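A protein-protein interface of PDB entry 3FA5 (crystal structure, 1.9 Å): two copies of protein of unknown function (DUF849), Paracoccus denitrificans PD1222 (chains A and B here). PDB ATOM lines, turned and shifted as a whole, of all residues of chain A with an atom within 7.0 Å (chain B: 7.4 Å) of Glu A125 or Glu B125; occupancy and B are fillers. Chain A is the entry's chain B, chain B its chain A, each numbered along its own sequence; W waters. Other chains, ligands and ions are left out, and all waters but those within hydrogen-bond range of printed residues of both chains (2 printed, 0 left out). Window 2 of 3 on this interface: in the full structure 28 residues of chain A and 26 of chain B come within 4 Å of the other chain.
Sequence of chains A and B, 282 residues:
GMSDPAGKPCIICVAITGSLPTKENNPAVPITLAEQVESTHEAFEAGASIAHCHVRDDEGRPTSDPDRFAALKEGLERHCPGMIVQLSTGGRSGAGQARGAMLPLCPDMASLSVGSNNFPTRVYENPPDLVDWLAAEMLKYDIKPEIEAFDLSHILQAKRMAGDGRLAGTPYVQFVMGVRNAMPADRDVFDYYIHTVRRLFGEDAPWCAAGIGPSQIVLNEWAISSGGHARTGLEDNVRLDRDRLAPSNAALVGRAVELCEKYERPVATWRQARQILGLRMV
The side-chain amide oxygen (OD1) of Asn B118 sits at hydrogen-bond distance from the side-chain hydroxyl (OG) of Ser A116, at 2.7 Å.
The side-chain carboxylate of Glu B125 lies close to the side-chain carboxylate of Glu A125, 3.4 Å away.
The side-chain amide oxygen (OD1) of Asn A118 is in hydrogen-bond range of the side-chain hydroxyl (OG) of Ser B116, at 2.6 Å.
ND2 of Asn A118 is in hydrogen-bond range of O of Asn B126 (2.8 Å).
O of Asn A126 lies within hydrogen-bond range of ND2 of Asn B118.
O of Glu A125 sits at hydrogen-bond distance from NH1 of Arg A99.
O of Gly A115 lies within hydrogen-bond range of ND2 of Asn A126 (3.2 Å).
The guanidinium group of Arg B99 lies within hydrogen-bond range of the backbone carbonyl oxygen of Glu B125 (3.3 Å).
The backbone NH (N) of Tyr B124 sits at hydrogen-bond distance from the backbone carbonyl oxygen (O) of Asn B117 (2.7 Å).
OD1 of Asn B126 sits at hydrogen-bond distance from NH2 of Arg B99, at 2.8 Å.
NH2 of Arg A99 sits at hydrogen-bond distance from OD1 of Asn A126 (2.8 Å).
Among the printed residues, pairs that only touch across the chains: Pro A127 with Val B123 (3.5 Å), Ser A116 with Val B123 (3.5 Å), Val A123 with Ser B116 (3.6 Å), Asn A118 with Gly B115 (3.6 Å), Val A123 with Pro B127 (3.7 Å), Ser A116 with Ser B116 (3.7 Å), Asn A117 with Ser B116 (3.8 Å), Asn A126 with Val B123 (3.8 Å), Ser A116 with Asn B117 (3.8 Å) and Gly A115 with Asn B118 (3.9 Å).
Glu A125 touches just one residue of chain B: Glu B125 (3.4 Å).
Of chain A, only Glu A125 comes within 4 Å of Glu B125.
Printed residues of chain B within 4 Å of Asn A117: Ser B116 (3.8 Å).
Of the printed residues of chain A, Ser B116 touches Ser A116 (3.7 Å), Asn A117 (3.8 Å), Asn A118 (2.6 Å) and Val A123 (3.6 Å).
Of the printed residues of chain B, Asn A126 touches Asn B118 and Val B123.
The nearest residue of chain A that does not touch Glu B125 is Val A123 (4.3 Å).
The nearest printed residue of chain B that does not touch Ser A116 is Tyr B124 (5.8 Å).
Hydrophobic or aromatic side chains of chain B within 4 Å of the printed part of chain A: Val B123 and Pro B127.
Printed residues of chain A that touch a printed residue of chain B: Gly A115, Ser A116, Asn A117, Asn A118, Val A123, Glu A125, Asn A126 and Pro A127.
Hydrophobic or aromatic side chains of chain A within 4 Å of the printed part of chain B: Val A123 and Pro A127.
Among the printed residues, 15 pairs touch across the chains.
Among the printed residues, no Asp or Glu carboxylate lies within 4 Å of a Lys or Arg side-chain nitrogen of the other chain.
Ser A116 touches its own counterpart, Ser B116.
Ser A116 touches Asn B118, and with the chains exchanged Asn A118 touches Ser B116.
Glu B125 touches its own counterpart, Glu A125.
Asn A126 touches Val B123, but with the chains exchanged Val A123 does not touch Asn B126 (4.04 Å).
Positions printed for both chains: 91, 99, 113, 115, 116, 117, 118, 119, 122, 123, 124, 125, 126, 127, 130 and 131.
Of the 15 pairs that touch across the chains among the printed residues, 14 have their exchanged pair printed and touching as well.
Water W2 bridges the backbone NH (N) of Ser B116 and the backbone NH (N) of Asn A118.
Water W1 lies within hydrogen-bond range of N of Ser A116 (2.9 Å) and N of Asn B118 (3.0 Å).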
ATOM      1  N   GLY A  91      -0.968  20.426 -11.039  1.00  0.00           N
ATOM      2  CA  GLY A  91      -0.010  20.874 -10.008  1.00  0.00           C
ATOM      3  C   GLY A  91       0.892  19.811  -9.385  1.00  0.00           C
ATOM      4  O   GLY A  91       1.833  20.150  -8.651  1.00  0.00           O
ATOM      5  N   ARG A  99       3.038  25.785 -14.437  1.00  0.00           N
ATOM      6  CA  ARG A  99       1.906  24.918 -14.835  1.00  0.00           C
ATOM      7  C   ARG A  99       1.132  25.391 -16.089  1.00  0.00           C
ATOM      8  O   ARG A  99       0.317  24.624 -16.614  1.00  0.00           O
ATOM      9  CB  ARG A  99       0.900  24.749 -13.668  1.00  0.00           C
ATOM     10  CG  ARG A  99       1.502  24.143 -12.380  1.00  0.00           C
ATOM     11  CD  ARG A  99       0.590  24.354 -11.134  1.00  0.00           C
ATOM     12  NE  ARG A  99      -0.709  23.716 -11.328  1.00  0.00           N
ATOM     13  CZ  ARG A  99      -1.730  23.730 -10.462  1.00  0.00           C
ATOM     14  NH1 ARG A  99      -1.662  24.366  -9.290  1.00  0.00           N
ATOM     15  NH2 ARG A  99      -2.840  23.091 -10.798  1.00  0.00           N
ATOM     16  N   SER A 113      -8.122  23.447 -12.714  1.00  0.00           N
ATOM     17  CA  SER A 113      -8.724  23.451 -11.400  1.00  0.00           C
ATOM     18  C   SER A 113      -9.007  24.906 -11.014  1.00  0.00           C
ATOM     19  O   SER A 113      -8.190  25.829 -11.288  1.00  0.00           O
ATOM     20  CB  SER A 113      -7.817  22.739 -10.389  1.00  0.00           C
ATOM     21  OG  SER A 113      -8.111  21.328 -10.351  1.00  0.00           O
ATOM     22  N   GLY A 115     -10.599  25.377  -7.740  1.00  0.00           N
ATOM     23  CA  GLY A 115     -10.635  25.343  -6.267  1.00  0.00           C
ATOM     24  C   GLY A 115      -9.499  24.472  -5.727  1.00  0.00           C
ATOM     25  O   GLY A 115      -8.824  23.807  -6.499  1.00  0.00           O
ATOM     26  N   SER A 116      -9.256  24.496  -4.410  1.00  0.00           N
ATOM     27  CA  SER A 116      -8.332  23.552  -3.804  1.00  0.00           C
ATOM     28  C   SER A 116      -9.137  22.467  -3.030  1.00  0.00           C
ATOM     29  O   SER A 116     -10.383  22.526  -2.909  1.00  0.00           O
ATOM     30  CB  SER A 116      -7.278  24.277  -2.940  1.00  0.00           C
ATOM     31  OG  SER A 116      -6.509  25.236  -3.692  1.00  0.00           O
ATOM     32  N   ASN A 117      -8.433  21.420  -2.620  1.00  0.00           N
ATOM     33  CA  ASN A 117      -9.070  20.261  -1.966  1.00  0.00           C
ATOM     34  C   ASN A 117      -7.973  19.357  -1.445  1.00  0.00           C
ATOM     35  O   ASN A 117      -6.827  19.456  -1.878  1.00  0.00           O
ATOM     36  CB  ASN A 117      -9.983  19.465  -2.921  1.00  0.00           C
ATOM     37  CG  ASN A 117      -9.264  19.040  -4.196  1.00  0.00           C
ATOM     38  OD1 ASN A 117      -9.219  19.797  -5.163  1.00  0.00           O
ATOM     39  ND2 ASN A 117      -8.672  17.857  -4.179  1.00  0.00           N
ATOM     40  N   ASN A 118      -8.323  18.461  -0.542  1.00  0.00           N
ATOM     41  CA  ASN A 118      -7.357  17.446  -0.138  1.00  0.00           C
ATOM     42  C   ASN A 118      -7.239  16.345  -1.207  1.00  0.00           C
ATOM     43  O   ASN A 118      -8.143  16.167  -2.068  1.00  0.00           O
ATOM     44  CB  ASN A 118      -7.676  16.910   1.247  1.00  0.00           C
ATOM     45  CG  ASN A 118      -7.254  17.875   2.347  1.00  0.00           C
ATOM     46  OD1 ASN A 118      -6.549  18.861   2.081  1.00  0.00           O
ATOM     47  ND2 ASN A 118      -7.654  17.590   3.588  1.00  0.00           N
ATOM     48  N   PHE A 119      -6.062  15.723  -1.203  1.00  0.00           N
ATOM     49  CA  PHE A 119      -5.673  14.561  -1.996  1.00  0.00           C
ATOM     50  C   PHE A 119      -5.250  13.473  -1.002  1.00  0.00           C
ATOM     51  O   PHE A 119      -5.215  13.701   0.223  1.00  0.00           O
ATOM     52  CB  PHE A 119      -4.476  14.890  -2.923  1.00  0.00           C
ATOM     53  CG  PHE A 119      -4.857  15.218  -4.355  1.00  0.00           C
ATOM     54  CD1 PHE A 119      -6.171  15.427  -4.727  1.00  0.00           C
ATOM     55  CD2 PHE A 119      -3.880  15.398  -5.313  1.00  0.00           C
ATOM     56  CE1 PHE A 119      -6.487  15.768  -6.037  1.00  0.00           C
ATOM     57  CE2 PHE A 119      -4.204  15.752  -6.597  1.00  0.00           C
ATOM     58  CZ  PHE A 119      -5.499  15.944  -6.954  1.00  0.00           C
ATOM     59  N   ARG A 122      -1.847  14.703   0.610  1.00  0.00           N
ATOM     60  CA  ARG A 122      -1.531  16.107   0.695  1.00  0.00           C
ATOM     61  C   ARG A 122      -2.696  17.016   0.308  1.00  0.00           C
ATOM     62  O   ARG A 122      -3.768  16.549  -0.126  1.00  0.00           O
ATOM     63  CB  ARG A 122      -0.352  16.417  -0.239  1.00  0.00           C
ATOM     64  CG  ARG A 122      -0.658  16.243  -1.716  1.00  0.00           C
ATOM     65  CD  ARG A 122       0.516  16.647  -2.583  1.00  0.00           C
ATOM     66  NE  ARG A 122       0.155  16.623  -4.002  1.00  0.00           N
ATOM     67  CZ  ARG A 122      -0.290  17.658  -4.716  1.00  0.00           C
ATOM     68  NH1 ARG A 122      -0.447  18.861  -4.191  1.00  0.00           N
ATOM     69  NH2 ARG A 122      -0.583  17.485  -5.995  1.00  0.00           N
ATOM     70  N   VAL A 123      -2.454  18.320   0.445  1.00  0.00           N
ATOM     71  CA  VAL A 123      -3.353  19.311  -0.108  1.00  0.00           C
ATOM     72  C   VAL A 123      -3.055  19.461  -1.599  1.00  0.00           C
ATOM     73  O   VAL A 123      -1.893  19.475  -2.002  1.00  0.00           O
ATOM     74  CB  VAL A 123      -3.202  20.667   0.574  1.00  0.00           C
ATOM     75  CG1 VAL A 123      -4.285  21.681   0.009  1.00  0.00           C
ATOM     76  CG2 VAL A 123      -3.300  20.499   2.101  1.00  0.00           C
ATOM     77  N   TYR A 124      -4.109  19.570  -2.419  1.00  0.00           N
ATOM     78  CA  TYR A 124      -3.953  19.929  -3.821  1.00  0.00           C
ATOM     79  C   TYR A 124      -4.167  21.448  -3.922  1.00  0.00           C
ATOM     80  O   TYR A 124      -5.294  21.908  -3.839  1.00  0.00           O
ATOM     81  CB  TYR A 124      -4.937  19.140  -4.689  1.00  0.00           C
ATOM     82  CG  TYR A 124      -4.767  19.305  -6.174  1.00  0.00           C
ATOM     83  CD1 TYR A 124      -3.513  19.254  -6.752  1.00  0.00           C
ATOM     84  CD2 TYR A 124      -5.857  19.487  -7.005  1.00  0.00           C
ATOM     85  CE1 TYR A 124      -3.349  19.388  -8.097  1.00  0.00           C
ATOM     86  CE2 TYR A 124      -5.698  19.611  -8.371  1.00  0.00           C
ATOM     87  CZ  TYR A 124      -4.442  19.559  -8.907  1.00  0.00           C
ATOM     88  OH  TYR A 124      -4.254  19.694 -10.267  1.00  0.00           O
ATOM     89  N   GLU A 125      -3.069  22.204  -4.090  1.00  0.00           N
ATOM     90  CA  GLU A 125      -3.059  23.652  -3.957  1.00  0.00           C
ATOM     91  C   GLU A 125      -3.314  24.308  -5.289  1.00  0.00           C
ATOM     92  O   GLU A 125      -2.596  24.079  -6.257  1.00  0.00           O
ATOM     93  CB  GLU A 125      -1.726  24.141  -3.404  1.00  0.00           C
ATOM     94  CG  GLU A 125      -1.430  23.653  -2.007  1.00  0.00           C
ATOM     95  CD  GLU A 125      -0.050  24.054  -1.506  1.00  0.00           C
ATOM     96  OE1 GLU A 125       0.549  25.002  -2.057  1.00  0.00           O
ATOM     97  OE2 GLU A 125       0.442  23.437  -0.538  1.00  0.00           O
ATOM     98  N   ASN A 126      -4.370  25.097  -5.334  1.00  0.00           N
ATOM     99  CA  ASN A 126      -4.693  25.888  -6.501  1.00  0.00           C
ATOM    100  C   ASN A 126      -4.994  27.313  -6.073  1.00  0.00           C
ATOM    101  O   ASN A 126      -6.139  27.751  -6.063  1.00  0.00           O
ATOM    102  CB  ASN A 126      -5.848  25.252  -7.225  1.00  0.00           C
ATOM    103  CG  ASN A 126      -5.447  23.936  -7.881  1.00  0.00           C
ATOM    104  OD1 ASN A 126      -4.667  23.945  -8.842  1.00  0.00           O
ATOM    105  ND2 ASN A 126      -5.959  22.800  -7.359  1.00  0.00           N
ATOM    106  N   PRO A 127      -3.955  28.053  -5.709  1.00  0.00           N
ATOM    107  CA  PRO A 127      -4.218  29.393  -5.221  1.00  0.00           C
ATOM    108  C   PRO A 127      -5.037  30.205  -6.180  1.00  0.00           C
ATOM    109  O   PRO A 127      -4.865  30.102  -7.384  1.00  0.00           O
ATOM    110  CB  PRO A 127      -2.828  30.024  -5.067  1.00  0.00           C
ATOM    111  CG  PRO A 127      -1.878  28.950  -5.120  1.00  0.00           C
ATOM    112  CD  PRO A 127      -2.517  27.827  -5.925  1.00  0.00           C
ATOM    113  N   LEU A 130      -3.267  32.064  -9.140  1.00  0.00           N
ATOM    114  CA  LEU A 130      -2.920  31.090 -10.164  1.00  0.00           C
ATOM    115  C   LEU A 130      -4.133  30.691 -10.992  1.00  0.00           C
ATOM    116  O   LEU A 130      -4.077  30.648 -12.223  1.00  0.00           O
ATOM    117  CB  LEU A 130      -2.312  29.858  -9.542  1.00  0.00           C
ATOM    118  CG  LEU A 130      -1.716  28.849 -10.527  1.00  0.00           C
ATOM    119  CD1 LEU A 130      -0.538  29.455 -11.350  1.00  0.00           C
ATOM    120  CD2 LEU A 130      -1.264  27.624  -9.751  1.00  0.00           C
ATOM    121  N   VAL A 131      -5.234  30.386 -10.317  1.00  0.00           N
ATOM    122  CA  VAL A 131      -6.450  30.017 -11.023  1.00  0.00           C
ATOM    123  C   VAL A 131      -6.808  31.121 -12.032  1.00  0.00           C
ATOM    124  O   VAL A 131      -7.037  30.877 -13.210  1.00  0.00           O
ATOM    125  CB  VAL A 131      -7.612  29.739 -10.051  1.00  0.00           C
ATOM    126  CG1 VAL A 131      -8.931  29.587 -10.858  1.00  0.00           C
ATOM    127  CG2 VAL A 131      -7.264  28.508  -9.199  1.00  0.00           C
ATOM    128  N   GLY B  90      -7.694  27.136  14.075  1.00  0.00           N
ATOM    129  CA  GLY B  90      -7.590  27.778  12.763  1.00  0.00           C
ATOM    130  C   GLY B  90      -6.173  27.960  12.259  1.00  0.00           C
ATOM    131  O   GLY B  90      -5.234  28.132  13.040  1.00  0.00           O
ATOM    132  N   GLY B  91      -6.041  27.896  10.935  1.00  0.00           N
ATOM    133  CA  GLY B  91      -4.738  27.905  10.235  1.00  0.00           C
ATOM    134  C   GLY B  91      -4.195  29.277   9.883  1.00  0.00           C
ATOM    135  O   GLY B  91      -3.082  29.382   9.389  1.00  0.00           O
ATOM    136  N   ARG B  92      -4.989  30.320  10.150  1.00  0.00           N
ATOM    137  CA  ARG B  92      -4.532  31.721  10.061  1.00  0.00           C
ATOM    138  C   ARG B  92      -3.699  32.157  11.267  1.00  0.00           C
ATOM    139  O   ARG B  92      -2.859  33.033  11.145  1.00  0.00           O
ATOM    140  CB  ARG B  92      -5.707  32.682   9.902  1.00  0.00           C
ATOM    141  CG  ARG B  92      -6.316  32.699   8.509  1.00  0.00           C
ATOM    142  CD  ARG B  92      -7.009  34.022   8.198  1.00  0.00           C
ATOM    143  NE  ARG B  92      -8.469  33.938   8.073  1.00  0.00           N
ATOM    144  CZ  ARG B  92      -9.171  34.159   6.959  1.00  0.00           C
ATOM    145  NH1 ARG B  92      -8.576  34.482   5.825  1.00  0.00           N
ATOM    146  NH2 ARG B  92     -10.503  34.061   6.985  1.00  0.00           N
ATOM    147  N   GLY B  94      -1.748  29.981  13.152  1.00  0.00           N
ATOM    148  CA  GLY B  94      -0.722  28.970  13.448  1.00  0.00           C
ATOM    149  C   GLY B  94      -0.583  27.985  12.297  1.00  0.00           C
ATOM    150  O   GLY B  94      -1.488  27.924  11.437  1.00  0.00           O
ATOM    151  N   GLY B  96       0.642  23.774  11.239  1.00  0.00           N
ATOM    152  CA  GLY B  96       0.906  22.424  11.737  1.00  0.00           C
ATOM    153  C   GLY B  96       0.388  22.183  13.149  1.00  0.00           C
ATOM    154  O   GLY B  96      -0.621  22.720  13.540  1.00  0.00           O
ATOM    155  N   ARG B  99      -1.413  24.537  15.852  1.00  0.00           N
ATOM    156  CA  ARG B  99      -2.832  24.814  15.827  1.00  0.00           C
ATOM    157  C   ARG B  99      -3.640  23.949  16.819  1.00  0.00           C
ATOM    158  O   ARG B  99      -4.856  24.109  16.969  1.00  0.00           O
ATOM    159  CB  ARG B  99      -3.325  24.579  14.402  1.00  0.00           C
ATOM    160  CG  ARG B  99      -2.712  25.508  13.365  1.00  0.00           C
ATOM    161  CD  ARG B  99      -3.006  25.019  11.969  1.00  0.00           C
ATOM    162  NE  ARG B  99      -4.441  24.940  11.740  1.00  0.00           N
ATOM    163  CZ  ARG B  99      -4.989  24.594  10.585  1.00  0.00           C
ATOM    164  NH1 ARG B  99      -4.222  24.285   9.540  1.00  0.00           N
ATOM    165  NH2 ARG B  99      -6.320  24.558  10.484  1.00  0.00           N
ATOM    166  N   SER B 113     -11.340  21.747  10.890  1.00  0.00           N
ATOM    167  CA  SER B 113     -11.480  21.673   9.439  1.00  0.00           C
ATOM    168  C   SER B 113     -11.004  20.271   9.099  1.00  0.00           C
ATOM    169  O   SER B 113      -9.982  19.757   9.663  1.00  0.00           O
ATOM    170  CB  SER B 113     -10.664  22.775   8.729  1.00  0.00           C
ATOM    171  OG  SER B 113     -11.371  24.014   8.693  1.00  0.00           O
ATOM    172  N   GLY B 115     -11.098  19.290   5.690  1.00  0.00           N
ATOM    173  CA  GLY B 115     -10.746  19.378   4.285  1.00  0.00           C
ATOM    174  C   GLY B 115     -10.031  20.689   4.025  1.00  0.00           C
ATOM    175  O   GLY B 115      -9.908  21.523   4.933  1.00  0.00           O
ATOM    176  N   SER B 116      -9.572  20.863   2.784  1.00  0.00           N
ATOM    177  CA  SER B 116      -8.972  22.102   2.355  1.00  0.00           C
ATOM    178  C   SER B 116      -9.873  22.754   1.299  1.00  0.00           C
ATOM    179  O   SER B 116     -10.807  22.135   0.791  1.00  0.00           O
ATOM    180  CB  SER B 116      -7.528  21.891   1.893  1.00  0.00           C
ATOM    181  OG  SER B 116      -6.703  21.310   2.940  1.00  0.00           O
ATOM    182  N   ASN B 117      -9.637  24.037   1.060  1.00  0.00           N
ATOM    183  CA  ASN B 117     -10.425  24.824   0.147  1.00  0.00           C
ATOM    184  C   ASN B 117      -9.714  26.141  -0.031  1.00  0.00           C
ATOM    185  O   ASN B 117      -8.730  26.437   0.661  1.00  0.00           O
ATOM    186  CB  ASN B 117     -11.819  25.079   0.713  1.00  0.00           C
ATOM    187  CG  ASN B 117     -11.776  25.689   2.113  1.00  0.00           C
ATOM    188  OD1 ASN B 117     -11.646  24.973   3.107  1.00  0.00           O
ATOM    189  ND2 ASN B 117     -11.854  27.014   2.188  1.00  0.00           N
ATOM    190  N   ASN B 118     -10.196  26.928  -0.974  1.00  0.00           N
ATOM    191  CA  ASN B 118      -9.632  28.239  -1.197  1.00  0.00           C
ATOM    192  C   ASN B 118     -10.298  29.240  -0.278  1.00  0.00           C
ATOM    193  O   ASN B 118     -11.387  29.006   0.264  1.00  0.00           O
ATOM    194  CB  ASN B 118      -9.747  28.649  -2.668  1.00  0.00           C
ATOM    195  CG  ASN B 118      -8.585  28.137  -3.508  1.00  0.00           C
ATOM    196  OD1 ASN B 118      -7.578  27.596  -2.983  1.00  0.00           O
ATOM    197  ND2 ASN B 118      -8.688  28.353  -4.825  1.00  0.00           N
ATOM    198  N   PHE B 119      -9.596  30.346  -0.105  1.00  0.00           N
ATOM    199  CA  PHE B 119     -10.008  31.451   0.730  1.00  0.00           C
ATOM    200  C   PHE B 119      -9.895  32.701  -0.129  1.00  0.00           C
ATOM    201  O   PHE B 119      -9.448  32.629  -1.264  1.00  0.00           O
ATOM    202  CB  PHE B 119      -9.063  31.504   1.928  1.00  0.00           C
ATOM    203  CG  PHE B 119      -9.641  30.981   3.223  1.00  0.00           C
ATOM    204  CD1 PHE B 119     -10.844  30.252   3.278  1.00  0.00           C
ATOM    205  CD2 PHE B 119      -8.929  31.194   4.420  1.00  0.00           C
ATOM    206  CE1 PHE B 119     -11.337  29.781   4.505  1.00  0.00           C
ATOM    207  CE2 PHE B 119      -9.428  30.731   5.632  1.00  0.00           C
ATOM    208  CZ  PHE B 119     -10.647  30.034   5.667  1.00  0.00           C
ATOM    209  N   ARG B 122      -5.842  33.189  -0.667  1.00  0.00           N
ATOM    210  CA  ARG B 122      -4.889  32.095  -0.533  1.00  0.00           C
ATOM    211  C   ARG B 122      -5.604  30.747  -0.431  1.00  0.00           C
ATOM    212  O   ARG B 122      -6.836  30.710  -0.348  1.00  0.00           O
ATOM    213  CB  ARG B 122      -4.027  32.317   0.714  1.00  0.00           C
ATOM    214  CG  ARG B 122      -4.814  32.492   2.031  1.00  0.00           C
ATOM    215  CD  ARG B 122      -3.985  31.986   3.228  1.00  0.00           C
ATOM    216  NE  ARG B 122      -4.795  31.680   4.413  1.00  0.00           N
ATOM    217  CZ  ARG B 122      -4.597  30.647   5.244  1.00  0.00           C
ATOM    218  NH1 ARG B 122      -3.620  29.761   5.043  1.00  0.00           N
ATOM    219  NH2 ARG B 122      -5.398  30.485   6.295  1.00  0.00           N
ATOM    220  N   VAL B 123      -4.833  29.659  -0.486  1.00  0.00           N
ATOM    221  CA  VAL B 123      -5.356  28.314  -0.244  1.00  0.00           C
ATOM    222  C   VAL B 123      -5.492  28.143   1.305  1.00  0.00           C
ATOM    223  O   VAL B 123      -4.585  28.516   2.043  1.00  0.00           O
ATOM    224  CB  VAL B 123      -4.392  27.212  -0.763  1.00  0.00           C
ATOM    225  CG1 VAL B 123      -4.950  25.790  -0.373  1.00  0.00           C
ATOM    226  CG2 VAL B 123      -4.110  27.342  -2.307  1.00  0.00           C
ATOM    227  N   TYR B 124      -6.586  27.559   1.783  1.00  0.00           N
ATOM    228  CA  TYR B 124      -6.759  27.332   3.220  1.00  0.00           C
ATOM    229  C   TYR B 124      -6.289  25.943   3.447  1.00  0.00           C
ATOM    230  O   TYR B 124      -6.982  25.038   3.174  1.00  0.00           O
ATOM    231  CB  TYR B 124      -8.229  27.517   3.677  1.00  0.00           C
ATOM    232  CG  TYR B 124      -8.438  27.370   5.196  1.00  0.00           C
ATOM    233  CD1 TYR B 124      -7.538  27.940   6.081  1.00  0.00           C
ATOM    234  CD2 TYR B 124      -9.517  26.660   5.743  1.00  0.00           C
ATOM    235  CE1 TYR B 124      -7.679  27.820   7.451  1.00  0.00           C
ATOM    236  CE2 TYR B 124      -9.680  26.552   7.148  1.00  0.00           C
ATOM    237  CZ  TYR B 124      -8.723  27.127   7.978  1.00  0.00           C
ATOM    238  OH  TYR B 124      -8.765  27.104   9.342  1.00  0.00           O
ATOM    239  N   GLU B 125      -5.058  25.766   3.888  1.00  0.00           N
ATOM    240  CA  GLU B 125      -4.519  24.425   3.910  1.00  0.00           C
ATOM    241  C   GLU B 125      -4.816  23.641   5.184  1.00  0.00           C
ATOM    242  O   GLU B 125      -4.510  24.104   6.285  1.00  0.00           O
ATOM    243  CB  GLU B 125      -3.004  24.489   3.710  1.00  0.00           C
ATOM    244  CG  GLU B 125      -2.601  25.182   2.428  1.00  0.00           C
ATOM    245  CD  GLU B 125      -1.187  25.647   2.495  1.00  0.00           C
ATOM    246  OE1 GLU B 125      -0.297  24.778   2.443  1.00  0.00           O
ATOM    247  OE2 GLU B 125      -0.980  26.869   2.669  1.00  0.00           O
ATOM    248  N   ASN B 126      -5.347  22.422   4.999  1.00  0.00           N
ATOM    249  CA  ASN B 126      -5.632  21.472   6.057  1.00  0.00           C
ATOM    250  C   ASN B 126      -5.240  20.079   5.625  1.00  0.00           C
ATOM    251  O   ASN B 126      -6.068  19.304   5.202  1.00  0.00           O
ATOM    252  CB  ASN B 126      -7.122  21.553   6.370  1.00  0.00           C
ATOM    253  CG  ASN B 126      -7.480  22.837   7.056  1.00  0.00           C
ATOM    254  OD1 ASN B 126      -7.044  23.060   8.188  1.00  0.00           O
ATOM    255  ND2 ASN B 126      -8.283  23.707   6.382  1.00  0.00           N
ATOM    256  N   PRO B 127      -3.947  19.753   5.705  1.00  0.00           N
ATOM    257  CA  PRO B 127      -3.499  18.490   5.155  1.00  0.00           C
ATOM    258  C   PRO B 127      -4.056  17.314   5.930  1.00  0.00           C
ATOM    259  O   PRO B 127      -4.251  17.400   7.152  1.00  0.00           O
ATOM    260  CB  PRO B 127      -1.977  18.546   5.250  1.00  0.00           C
ATOM    261  CG  PRO B 127      -1.616  19.856   5.911  1.00  0.00           C
ATOM    262  CD  PRO B 127      -2.868  20.618   6.190  1.00  0.00           C
ATOM    263  N   LEU B 130      -2.497  16.336   9.287  1.00  0.00           N
ATOM    264  CA  LEU B 130      -2.737  17.311  10.360  1.00  0.00           C
ATOM    265  C   LEU B 130      -4.175  17.197  10.899  1.00  0.00           C
ATOM    266  O   LEU B 130      -4.380  17.257  12.108  1.00  0.00           O
ATOM    267  CB  LEU B 130      -2.445  18.765   9.920  1.00  0.00           C
ATOM    268  CG  LEU B 130      -2.726  19.824  11.007  1.00  0.00           C
ATOM    269  CD1 LEU B 130      -1.767  19.593  12.158  1.00  0.00           C
ATOM    270  CD2 LEU B 130      -2.664  21.262  10.516  1.00  0.00           C
ATOM    271  N   VAL B 131      -5.130  17.040   9.994  1.00  0.00           N
ATOM    272  CA  VAL B 131      -6.563  16.849  10.318  1.00  0.00           C
ATOM    273  C   VAL B 131      -6.742  15.655  11.278  1.00  0.00           C
ATOM    274  O   VAL B 131      -7.534  15.712  12.251  1.00  0.00           O
ATOM    275  CB  VAL B 131      -7.400  16.529   9.044  1.00  0.00           C
ATOM    276  CG1 VAL B 131      -8.761  15.944   9.409  1.00  0.00           C
ATOM    277  CG2 VAL B 131      -7.533  17.742   8.096  1.00  0.00           C
HETATM  278  O   HOH W   1     -11.693  25.451  -3.061  1.00  0.00           O
HETATM  279  O   HOH W   2     -10.687  19.218   0.829  1.00  0.00           O
